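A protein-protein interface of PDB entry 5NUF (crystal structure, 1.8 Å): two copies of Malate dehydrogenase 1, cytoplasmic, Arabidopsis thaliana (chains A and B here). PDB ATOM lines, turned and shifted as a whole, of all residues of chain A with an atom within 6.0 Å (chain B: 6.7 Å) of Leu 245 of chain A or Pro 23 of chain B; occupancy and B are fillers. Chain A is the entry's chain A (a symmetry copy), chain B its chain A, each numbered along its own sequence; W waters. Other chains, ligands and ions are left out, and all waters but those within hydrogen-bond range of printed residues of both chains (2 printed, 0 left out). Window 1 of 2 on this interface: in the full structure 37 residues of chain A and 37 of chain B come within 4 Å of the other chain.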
ATOM      1  N   GLN A  16     -15.089  19.384 -12.767  1.00  0.00           N
ATOM      2  CA  GLN A  16     -13.666  19.503 -12.435  1.00  0.00           C
ATOM      3  C   GLN A  16     -13.406  20.682 -11.509  1.00  0.00           C
ATOM      4  O   GLN A  16     -12.743  20.545 -10.451  1.00  0.00           O
ATOM      5  CB  GLN A  16     -12.901  19.680 -13.754  1.00  0.00           C
ATOM      6  CG  GLN A  16     -11.455  19.418 -13.585  1.00  0.00           C
ATOM      7  CD  GLN A  16     -10.515  19.914 -14.755  1.00  0.00           C
ATOM      8  OE1 GLN A  16      -9.348  19.539 -14.698  1.00  0.00           O
ATOM      9  NE2 GLN A  16     -11.007  20.738 -15.753  1.00  0.00           N
ATOM     10  N   ILE A  17     -13.915  21.855 -11.868  1.00  0.00           N
ATOM     11  CA  ILE A  17     -13.710  23.042 -11.017  1.00  0.00           C
ATOM     12  C   ILE A  17     -14.457  22.893  -9.712  1.00  0.00           C
ATOM     13  O   ILE A  17     -13.932  23.222  -8.642  1.00  0.00           O
ATOM     14  CB  ILE A  17     -14.091  24.331 -11.728  1.00  0.00           C
ATOM     15  CG1 ILE A  17     -13.110  24.614 -12.843  1.00  0.00           C
ATOM     16  CG2 ILE A  17     -14.128  25.501 -10.767  1.00  0.00           C
ATOM     17  CD1 ILE A  17     -13.512  25.744 -13.752  1.00  0.00           C
ATOM     18  N   ALA A  20     -12.407  20.814  -7.299  1.00  0.00           N
ATOM     19  CA  ALA A  20     -11.337  21.649  -6.749  1.00  0.00           C
ATOM     20  C   ALA A  20     -11.771  22.728  -5.779  1.00  0.00           C
ATOM     21  O   ALA A  20     -11.044  23.108  -4.860  1.00  0.00           O
ATOM     22  CB  ALA A  20     -10.568  22.289  -7.923  1.00  0.00           C
ATOM     23  N   MET A  24     -11.959  23.949  -0.867  1.00  0.00           N
ATOM     24  CA  MET A  24     -11.360  25.239  -0.521  1.00  0.00           C
ATOM     25  C   MET A  24     -12.376  26.101   0.292  1.00  0.00           C
ATOM     26  O   MET A  24     -12.020  26.716   1.308  1.00  0.00           O
ATOM     27  CB  MET A  24     -10.884  26.031  -1.750  1.00  0.00           C
ATOM     28  CG  MET A  24      -9.844  25.395  -2.608  1.00  0.00           C
ATOM     29  SD  MET A  24      -9.571  26.367  -4.114  1.00  0.00           S
ATOM     30  CE  MET A  24      -8.353  25.374  -4.961  1.00  0.00           C
ATOM     31  N   ARG A 239      -2.546  19.562 -20.296  1.00  0.00           N
ATOM     32  CA  ARG A 239      -3.297  18.654 -19.457  1.00  0.00           C
ATOM     33  C   ARG A 239      -4.414  17.901 -20.159  1.00  0.00           C
ATOM     34  O   ARG A 239      -4.965  16.987 -19.600  1.00  0.00           O
ATOM     35  CB  ARG A 239      -3.961  19.422 -18.270  1.00  0.00           C
ATOM     36  CG  ARG A 239      -2.979  20.063 -17.315  1.00  0.00           C
ATOM     37  CD  ARG A 239      -3.638  20.751 -16.155  1.00  0.00           C
ATOM     38  NE  ARG A 239      -4.521  19.795 -15.491  1.00  0.00           N
ATOM     39  CZ  ARG A 239      -5.829  19.903 -15.376  1.00  0.00           C
ATOM     40  NH1 ARG A 239      -6.471  21.037 -15.701  1.00  0.00           N
ATOM     41  NH2 ARG A 239      -6.481  18.920 -14.739  1.00  0.00           N
ATOM     42  N   SER A 243      -8.389  24.572 -17.102  1.00  0.00           N
ATOM     43  CA  SER A 243      -7.890  24.836 -15.768  1.00  0.00           C
ATOM     44  C   SER A 243      -8.942  24.547 -14.714  1.00  0.00           C
ATOM     45  O   SER A 243     -10.135  24.703 -14.957  1.00  0.00           O
ATOM     46  CB  SER A 243      -7.492  26.317 -15.661  1.00  0.00           C
ATOM     47  OG  SER A 243      -8.607  27.162 -15.839  1.00  0.00           O
ATOM     48  N   ALA A 244      -8.505  24.156 -13.543  1.00  0.00           N
ATOM     49  CA  ALA A 244      -9.456  23.839 -12.480  1.00  0.00           C
ATOM     50  C   ALA A 244      -8.912  24.224 -11.139  1.00  0.00           C
ATOM     51  O   ALA A 244      -9.528  25.019 -10.414  1.00  0.00           O
ATOM     52  CB  ALA A 244      -9.938  22.365 -12.548  1.00  0.00           C
ATOM     53  N   LEU A 245      -7.745  23.682 -10.766  1.00  0.00           N
ATOM     54  CA  LEU A 245      -7.104  24.070  -9.539  1.00  0.00           C
ATOM     55  C   LEU A 245      -6.955  25.597  -9.450  1.00  0.00           C
ATOM     56  O   LEU A 245      -7.292  26.220  -8.441  1.00  0.00           O
ATOM     57  CB  LEU A 245      -5.736  23.405  -9.544  1.00  0.00           C
ATOM     58  CG  LEU A 245      -4.572  23.734  -8.683  1.00  0.00           C
ATOM     59  CD1 LEU A 245      -3.562  22.574  -8.901  1.00  0.00           C
ATOM     60  CD2 LEU A 245      -3.957  25.117  -8.797  1.00  0.00           C
ATOM     61  N   SER A 246      -6.463  26.198 -10.517  1.00  0.00           N
ATOM     62  CA  SER A 246      -6.187  27.628 -10.550  1.00  0.00           C
ATOM     63  C   SER A 246      -7.487  28.473 -10.717  1.00  0.00           C
ATOM     64  O   SER A 246      -7.577  29.589 -10.201  1.00  0.00           O
ATOM     65  CB  SER A 246      -5.168  27.942 -11.653  1.00  0.00           C
ATOM     66  OG  SER A 246      -5.544  27.438 -12.957  1.00  0.00           O
ATOM     67  N   ALA A 247      -8.468  27.956 -11.445  1.00  0.00           N
ATOM     68  CA  ALA A 247      -9.783  28.597 -11.551  1.00  0.00           C
ATOM     69  C   ALA A 247     -10.507  28.613 -10.197  1.00  0.00           C
ATOM     70  O   ALA A 247     -10.999  29.668  -9.749  1.00  0.00           O
ATOM     71  CB  ALA A 247     -10.622  27.893 -12.616  1.00  0.00           C
ATOM     72  N   ALA A 248     -10.528  27.475  -9.520  1.00  0.00           N
ATOM     73  CA  ALA A 248     -11.083  27.403  -8.165  1.00  0.00           C
ATOM     74  C   ALA A 248     -10.400  28.351  -7.184  1.00  0.00           C
ATOM     75  O   ALA A 248     -11.054  29.080  -6.452  1.00  0.00           O
ATOM     76  CB  ALA A 248     -11.047  25.942  -7.620  1.00  0.00           C
ATOM     77  N   SER A 249      -9.076  28.333  -7.162  1.00  0.00           N
ATOM     78  CA  SER A 249      -8.336  29.179  -6.274  1.00  0.00           C
ATOM     79  C   SER A 249      -8.618  30.673  -6.581  1.00  0.00           C
ATOM     80  O   SER A 249      -8.815  31.483  -5.648  1.00  0.00           O
ATOM     81  CB  SER A 249      -6.845  28.902  -6.399  1.00  0.00           C
ATOM     82  OG  SER A 249      -6.132  29.680  -5.436  1.00  0.00           O
ATOM     83  N   SER A 250      -8.684  31.020  -7.857  1.00  0.00           N
ATOM     84  CA  SER A 250      -8.923  32.386  -8.239  1.00  0.00           C
ATOM     85  C   SER A 250     -10.399  32.801  -7.919  1.00  0.00           C
ATOM     86  O   SER A 250     -10.657  33.932  -7.575  1.00  0.00           O
ATOM     87  CB  SER A 250      -8.666  32.585  -9.701  1.00  0.00           C
ATOM     88  OG  SER A 250      -7.292  32.362  -9.999  1.00  0.00           O
ATOM     89  N   ILE B  17      -5.154  12.665  -6.503  1.00  0.00           N
ATOM     90  CA  ILE B  17      -4.889  13.210  -5.158  1.00  0.00           C
ATOM     91  C   ILE B  17      -3.878  14.330  -5.229  1.00  0.00           C
ATOM     92  O   ILE B  17      -4.033  15.365  -4.569  1.00  0.00           O
ATOM     93  CB  ILE B  17      -4.451  12.131  -4.179  1.00  0.00           C
ATOM     94  CG1 ILE B  17      -5.607  11.203  -3.883  1.00  0.00           C
ATOM     95  CG2 ILE B  17      -3.932  12.734  -2.890  1.00  0.00           C
ATOM     96  CD1 ILE B  17      -5.232   9.974  -3.100  1.00  0.00           C
ATOM     97  N   GLY B  18      -2.875  14.180  -6.058  1.00  0.00           N
ATOM     98  CA  GLY B  18      -1.904  15.177  -6.244  1.00  0.00           C
ATOM     99  C   GLY B  18      -2.464  16.547  -6.658  1.00  0.00           C
ATOM    100  O   GLY B  18      -2.098  17.603  -6.090  1.00  0.00           O
ATOM    101  N   TYR B  19      -3.384  16.493  -7.610  1.00  0.00           N
ATOM    102  CA  TYR B  19      -4.065  17.650  -8.089  1.00  0.00           C
ATOM    103  C   TYR B  19      -4.925  18.346  -7.024  1.00  0.00           C
ATOM    104  O   TYR B  19      -4.955  19.603  -6.975  1.00  0.00           O
ATOM    105  CB  TYR B  19      -4.921  17.277  -9.289  1.00  0.00           C
ATOM    106  CG  TYR B  19      -5.390  18.448 -10.125  1.00  0.00           C
ATOM    107  CD1 TYR B  19      -4.503  19.090 -10.969  1.00  0.00           C
ATOM    108  CD2 TYR B  19      -6.682  18.901 -10.048  1.00  0.00           C
ATOM    109  CE1 TYR B  19      -4.910  20.164 -11.785  1.00  0.00           C
ATOM    110  CE2 TYR B  19      -7.103  19.986 -10.800  1.00  0.00           C
ATOM    111  CZ  TYR B  19      -6.208  20.601 -11.708  1.00  0.00           C
ATOM    112  OH  TYR B  19      -6.643  21.702 -12.401  1.00  0.00           O
ATOM    113  N   ALA B  20      -5.617  17.557  -6.185  1.00  0.00           N
ATOM    114  CA  ALA B  20      -6.318  18.080  -5.011  1.00  0.00           C
ATOM    115  C   ALA B  20      -5.440  18.635  -3.908  1.00  0.00           C
ATOM    116  O   ALA B  20      -5.815  19.554  -3.178  1.00  0.00           O
ATOM    117  CB  ALA B  20      -7.216  16.963  -4.444  1.00  0.00           C
ATOM    118  N   LEU B  21      -4.241  18.046  -3.758  1.00  0.00           N
ATOM    119  CA  LEU B  21      -3.350  18.317  -2.657  1.00  0.00           C
ATOM    120  C   LEU B  21      -2.432  19.513  -2.816  1.00  0.00           C
ATOM    121  O   LEU B  21      -2.295  20.328  -1.890  1.00  0.00           O
ATOM    122  CB  LEU B  21      -2.470  17.077  -2.327  1.00  0.00           C
ATOM    123  CG  LEU B  21      -1.506  17.228  -1.179  1.00  0.00           C
ATOM    124  CD1 LEU B  21      -2.129  17.593   0.146  1.00  0.00           C
ATOM    125  CD2 LEU B  21      -0.723  15.928  -0.985  1.00  0.00           C
ATOM    126  N   VAL B  22      -1.786  19.606  -3.954  1.00  0.00           N
ATOM    127  CA  VAL B  22      -0.837  20.709  -4.107  1.00  0.00           C
ATOM    128  C   VAL B  22      -1.401  22.138  -3.878  1.00  0.00           C
ATOM    129  O   VAL B  22      -0.699  22.941  -3.317  1.00  0.00           O
ATOM    130  CB  VAL B  22       0.026  20.616  -5.407  1.00  0.00           C
ATOM    131  CG1 VAL B  22       0.822  19.321  -5.353  1.00  0.00           C
ATOM    132  CG2 VAL B  22      -0.812  20.708  -6.699  1.00  0.00           C
ATOM    133  N   PRO B  23      -2.643  22.443  -4.303  1.00  0.00           N
ATOM    134  CA  PRO B  23      -3.042  23.789  -4.010  1.00  0.00           C
ATOM    135  C   PRO B  23      -3.381  23.993  -2.524  1.00  0.00           C
ATOM    136  O   PRO B  23      -3.293  25.147  -2.022  1.00  0.00           O
ATOM    137  CB  PRO B  23      -4.316  23.997  -4.864  1.00  0.00           C
ATOM    138  CG  PRO B  23      -4.906  22.594  -4.959  1.00  0.00           C
ATOM    139  CD  PRO B  23      -3.683  21.713  -5.087  1.00  0.00           C
ATOM    140  N   MET B  24      -3.755  22.929  -1.818  1.00  0.00           N
ATOM    141  CA  MET B  24      -3.971  23.048  -0.375  1.00  0.00           C
ATOM    142  C   MET B  24      -2.628  23.392   0.342  1.00  0.00           C
ATOM    143  O   MET B  24      -2.579  24.267   1.218  1.00  0.00           O
ATOM    144  CB  MET B  24      -4.576  21.780   0.249  1.00  0.00           C
ATOM    145  CG  MET B  24      -5.908  21.342  -0.257  1.00  0.00           C
ATOM    146  SD  MET B  24      -6.356  19.725   0.431  1.00  0.00           S
ATOM    147  CE  MET B  24      -7.926  19.424  -0.365  1.00  0.00           C
ATOM    148  N   ILE B  25      -1.567  22.749  -0.089  1.00  0.00           N
ATOM    149  CA  ILE B  25      -0.242  23.034   0.469  1.00  0.00           C
ATOM    150  C   ILE B  25       0.131  24.508   0.159  1.00  0.00           C
ATOM    151  O   ILE B  25       0.606  25.256   1.051  1.00  0.00           O
ATOM    152  CB  ILE B  25       0.815  22.044  -0.043  1.00  0.00           C
ATOM    153  CG1 ILE B  25       0.535  20.612   0.404  1.00  0.00           C
ATOM    154  CG2 ILE B  25       2.222  22.460   0.361  1.00  0.00           C
ATOM    155  CD1 ILE B  25       1.282  19.550  -0.426  1.00  0.00           C
ATOM    156  N   ALA B  26      -0.081  24.910  -1.116  1.00  0.00           N
ATOM    157  CA  ALA B  26       0.282  26.245  -1.554  1.00  0.00           C
ATOM    158  C   ALA B  26      -0.492  27.328  -0.837  1.00  0.00           C
ATOM    159  O   ALA B  26       0.030  28.436  -0.692  1.00  0.00           O
ATOM    160  CB  ALA B  26       0.112  26.389  -3.022  1.00  0.00           C
ATOM    161  N   ARG B  27      -1.686  27.007  -0.387  1.00  0.00           N
ATOM    162  CA  ARG B  27      -2.508  27.950   0.374  1.00  0.00           C
ATOM    163  C   ARG B  27      -2.195  28.008   1.833  1.00  0.00           C
ATOM    164  O   ARG B  27      -2.738  28.848   2.475  1.00  0.00           O
ATOM    165  CB  ARG B  27      -4.015  27.540   0.280  1.00  0.00           C
ATOM    166  CG  ARG B  27      -4.755  27.993  -0.900  1.00  0.00           C
ATOM    167  CD  ARG B  27      -4.918  29.521  -0.844  1.00  0.00           C
ATOM    168  NE  ARG B  27      -5.747  29.941  -1.917  1.00  0.00           N
ATOM    169  CZ  ARG B  27      -5.838  31.172  -2.380  1.00  0.00           C
ATOM    170  NH1 ARG B  27      -5.019  32.144  -1.969  1.00  0.00           N
ATOM    171  NH2 ARG B  27      -6.721  31.372  -3.323  1.00  0.00           N
ATOM    172  N   GLY B  28      -1.337  27.147   2.366  1.00  0.00           N
ATOM    173  CA  GLY B  28      -1.019  27.224   3.796  1.00  0.00           C
ATOM    174  C   GLY B  28      -1.829  26.313   4.662  1.00  0.00           C
ATOM    175  O   GLY B  28      -1.638  26.305   5.859  1.00  0.00           O
ATOM    176  N   ILE B  29      -2.625  25.403   4.059  1.00  0.00           N
ATOM    177  CA  ILE B  29      -3.447  24.515   4.840  1.00  0.00           C
ATOM    178  C   ILE B  29      -2.662  23.413   5.533  1.00  0.00           C
ATOM    179  O   ILE B  29      -3.108  22.915   6.629  1.00  0.00           O
ATOM    180  CB  ILE B  29      -4.557  23.848   3.975  1.00  0.00           C
ATOM    181  CG1 ILE B  29      -5.436  24.976   3.485  1.00  0.00           C
ATOM    182  CG2 ILE B  29      -5.394  22.785   4.747  1.00  0.00           C
ATOM    183  CD1 ILE B  29      -6.153  24.602   2.277  1.00  0.00           C
ATOM    184  N   LEU B  39       7.243  23.768  -3.336  1.00  0.00           N
ATOM    185  CA  LEU B  39       6.713  22.482  -3.741  1.00  0.00           C
ATOM    186  C   LEU B  39       7.738  21.775  -4.624  1.00  0.00           C
ATOM    187  O   LEU B  39       8.262  22.386  -5.562  1.00  0.00           O
ATOM    188  CB  LEU B  39       5.405  22.625  -4.529  1.00  0.00           C
ATOM    189  CG  LEU B  39       4.156  22.794  -3.633  1.00  0.00           C
ATOM    190  CD1 LEU B  39       2.955  23.289  -4.454  1.00  0.00           C
ATOM    191  CD2 LEU B  39       3.869  21.418  -3.057  1.00  0.00           C
ATOM    192  N   VAL B  54       0.244  21.009 -14.262  1.00  0.00           N
ATOM    193  CA  VAL B  54      -0.006  21.322 -12.853  1.00  0.00           C
ATOM    194  C   VAL B  54       0.835  22.480 -12.354  1.00  0.00           C
ATOM    195  O   VAL B  54       0.325  23.360 -11.681  1.00  0.00           O
ATOM    196  CB  VAL B  54       0.120  20.089 -11.964  1.00  0.00           C
ATOM    197  CG1 VAL B  54      -0.189  20.454 -10.525  1.00  0.00           C
ATOM    198  CG2 VAL B  54      -0.796  19.003 -12.462  1.00  0.00           C
ATOM    199  N   GLU B  57      -0.505  25.707 -13.605  1.00  0.00           N
ATOM    200  CA  GLU B  57      -1.683  26.141 -12.815  1.00  0.00           C
ATOM    201  C   GLU B  57      -1.293  26.727 -11.476  1.00  0.00           C
ATOM    202  O   GLU B  57      -1.930  27.681 -11.011  1.00  0.00           O
ATOM    203  CB  GLU B  57      -2.684  24.989 -12.622  1.00  0.00           C
ATOM    204  CG  GLU B  57      -3.459  24.714 -13.926  1.00  0.00           C
ATOM    205  CD  GLU B  57      -4.802  24.106 -13.644  1.00  0.00           C
ATOM    206  OE1 GLU B  57      -5.682  24.831 -13.091  1.00  0.00           O
ATOM    207  OE2 GLU B  57      -4.991  22.890 -13.955  1.00  0.00           O
ATOM    208  N   LEU B  58      -0.253  26.128 -10.816  1.00  0.00           N
ATOM    209  CA  LEU B  58       0.166  26.625  -9.539  1.00  0.00           C
ATOM    210  C   LEU B  58       0.721  28.037  -9.680  1.00  0.00           C
ATOM    211  O   LEU B  58       0.469  28.899  -8.835  1.00  0.00           O
ATOM    212  CB  LEU B  58       1.231  25.708  -8.956  1.00  0.00           C
ATOM    213  CG  LEU B  58       0.747  24.346  -8.421  1.00  0.00           C
ATOM    214  CD1 LEU B  58       1.883  23.405  -8.147  1.00  0.00           C
ATOM    215  CD2 LEU B  58      -0.002  24.550  -7.104  1.00  0.00           C
ATOM    216  N   ILE B  59       1.466  28.278 -10.755  1.00  0.00           N
ATOM    217  CA  ILE B  59       1.963  29.627 -11.060  1.00  0.00           C
ATOM    218  C   ILE B  59       0.804  30.559 -11.322  1.00  0.00           C
ATOM    219  O   ILE B  59       0.806  31.677 -10.835  1.00  0.00           O
ATOM    220  CB  ILE B  59       2.903  29.560 -12.288  1.00  0.00           C
ATOM    221  CG1 ILE B  59       4.242  28.950 -11.840  1.00  0.00           C
ATOM    222  CG2 ILE B  59       3.131  30.904 -12.925  1.00  0.00           C
ATOM    223  CD1 ILE B  59       5.010  28.451 -13.051  1.00  0.00           C
ATOM    224  N   ALA B  61      -2.175  30.568 -10.237  1.00  0.00           N
ATOM    225  CA  ALA B  61      -2.973  30.896  -9.057  1.00  0.00           C
ATOM    226  C   ALA B  61      -2.414  32.022  -8.198  1.00  0.00           C
ATOM    227  O   ALA B  61      -3.118  32.542  -7.291  1.00  0.00           O
ATOM    228  CB  ALA B  61      -3.147  29.634  -8.207  1.00  0.00           C
ATOM    229  N   PHE B  63      -0.268  32.159  -5.686  1.00  0.00           N
ATOM    230  CA  PHE B  63      -0.306  31.817  -4.298  1.00  0.00           C
ATOM    231  C   PHE B  63       0.812  32.589  -3.512  1.00  0.00           C
ATOM    232  O   PHE B  63       2.006  32.324  -3.722  1.00  0.00           O
ATOM    233  CB  PHE B  63      -0.011  30.310  -4.115  1.00  0.00           C
ATOM    234  CG  PHE B  63      -1.131  29.374  -4.527  1.00  0.00           C
ATOM    235  CD1 PHE B  63      -2.339  29.352  -3.838  1.00  0.00           C
ATOM    236  CD2 PHE B  63      -0.948  28.485  -5.581  1.00  0.00           C
ATOM    237  CE1 PHE B  63      -3.344  28.500  -4.234  1.00  0.00           C
ATOM    238  CE2 PHE B  63      -1.924  27.608  -5.927  1.00  0.00           C
ATOM    239  CZ  PHE B  63      -3.102  27.600  -5.263  1.00  0.00           C
HETATM  240  O   HOH W   1      -5.524  31.941  -6.767  1.00  0.00           O
HETATM  241  O   HOH W   2      -7.028  28.092  -3.010  1.00  0.00           O
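The side-chain hydroxyl of Tyr 19 of chain B lies within hydrogen-bond range of the guanidinium group of Arg 239 of chain A, 3.4 Å away. The side-chain hydroxyl (OH) of Tyr 19 of chain B lies within hydrogen-bond range of the backbone NH (N) of Ala 244 of chain A, 3.3 Å away. The side-chain hydroxyl of Tyr 19 of chain B sits at hydrogen-bond distance from the backbone NH of Leu 245 of chain A, at 2.8 Å. The guanidinium group of Arg 27 of chain B sits at hydrogen-bond distance from the side-chain hydroxyl of Ser 249 of chain A, 2.8 Å away. The side-chain carboxylate (OE2) of Glu 57 of chain B is in salt-bridge range of the guanidinium group (NH1) of Arg 239 of chain A, 2.9 Å away. OE1 of Glu 57 of chain B lies within hydrogen-bond range of N of Ala 244 of chain A (2.9 Å). The side-chain carboxylate (OE1) of Glu 57 of chain B is in hydrogen-bond range of the backbone NH (N) of Leu 245 of chain A (3.3 Å). OG of Ser 246 of chain A lies within hydrogen-bond range of OE1 of Glu 57 of chain B, 2.6 Å away.
OH of Tyr 19 of chain B sits at hydrogen-bond distance from OE2 of Glu 57 of chain B. The side-chain amide oxygen of Gln 16 of chain A lies within hydrogen-bond range of the guanidinium group of Arg 239 of chain A (2.9 Å). The backbone NH of Ser 249 of chain A is in hydrogen-bond range of the side-chain sulfur of Met 24 of chain A (3.7 Å). OG of Ser 250 of chain A sits at hydrogen-bond distance from O of Ser 246 of chain A (2.8 Å).
OE1 of Glu 57 of chain B touches CA of Ser 243 of chain A, at 3.5 Å. Leu 245 of chain A touches Val 22 of chain B (CD1 to CG2, 3.99 Å). Leu 245 of chain A touches Pro 23 of chain B. CE1 of Phe 63 of chain B touches OG of Ser 249 of chain A (3.3 Å).
Of the printed residues of chain B, Leu 245 of chain A touches Tyr 19, Val 22, Pro 23 and Glu 57. Printed residues of chain A within 4 Å of Pro 23 of chain B: Leu 245 (3.8 Å). Of the printed residues of chain B, Arg 239 of chain A touches Tyr 19 (3.4 Å) and Glu 57 (2.9 Å). Of the printed residues of chain A, Val 22 of chain B touches Leu 245 (3.99 Å). Ala 20 of chain A touches none of the printed residues of chain B. The nearest printed residue of chain B that does not touch Leu 245 of chain A is Val 54 of chain B (4.3 Å). The nearest printed residue of chain A that does not touch Pro 23 of chain B is Met 24 of chain A (4.3 Å).
Printed residues of chain A that touch a printed residue of chain B: Arg 239, Ser 243, Ala 244, Leu 245, Ser 246 and Ser 249. Hydrophobic or aromatic side chains of chain A that line the printed part of chain B: Ala 244 and Leu 245. Hydrophobic or aromatic side chains of chain B within 4 Å of the printed part of chain A: Tyr 19, Val 22, Pro 23 and Phe 63. Among the printed residues, 12 pairs touch across the chains. Among the printed residues, Asp or Glu carboxylates within 4 Å of a Lys or Arg side-chain nitrogen of the other chain: Arg 239 of chain A with Glu 57 of chain B (2.9 Å).
3 positions are printed for both chains.
Water W2 lies within hydrogen-bond range of the guanidinium group of Arg 27 of chain B (2.5 Å), the side-chain hydroxyl of Ser 249 of chain A (3.0 Å) and the side-chain sulfur of Met 24 of chain A (3.3 Å). Water W1 lies within hydrogen-bond range of the backbone carbonyl oxygen of Ala 61 of chain B (2.5 Å), the side-chain hydroxyl of Ser 249 of chain A (2.7 Å) and the backbone NH of Ser 250 of chain A (3.5 Å).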
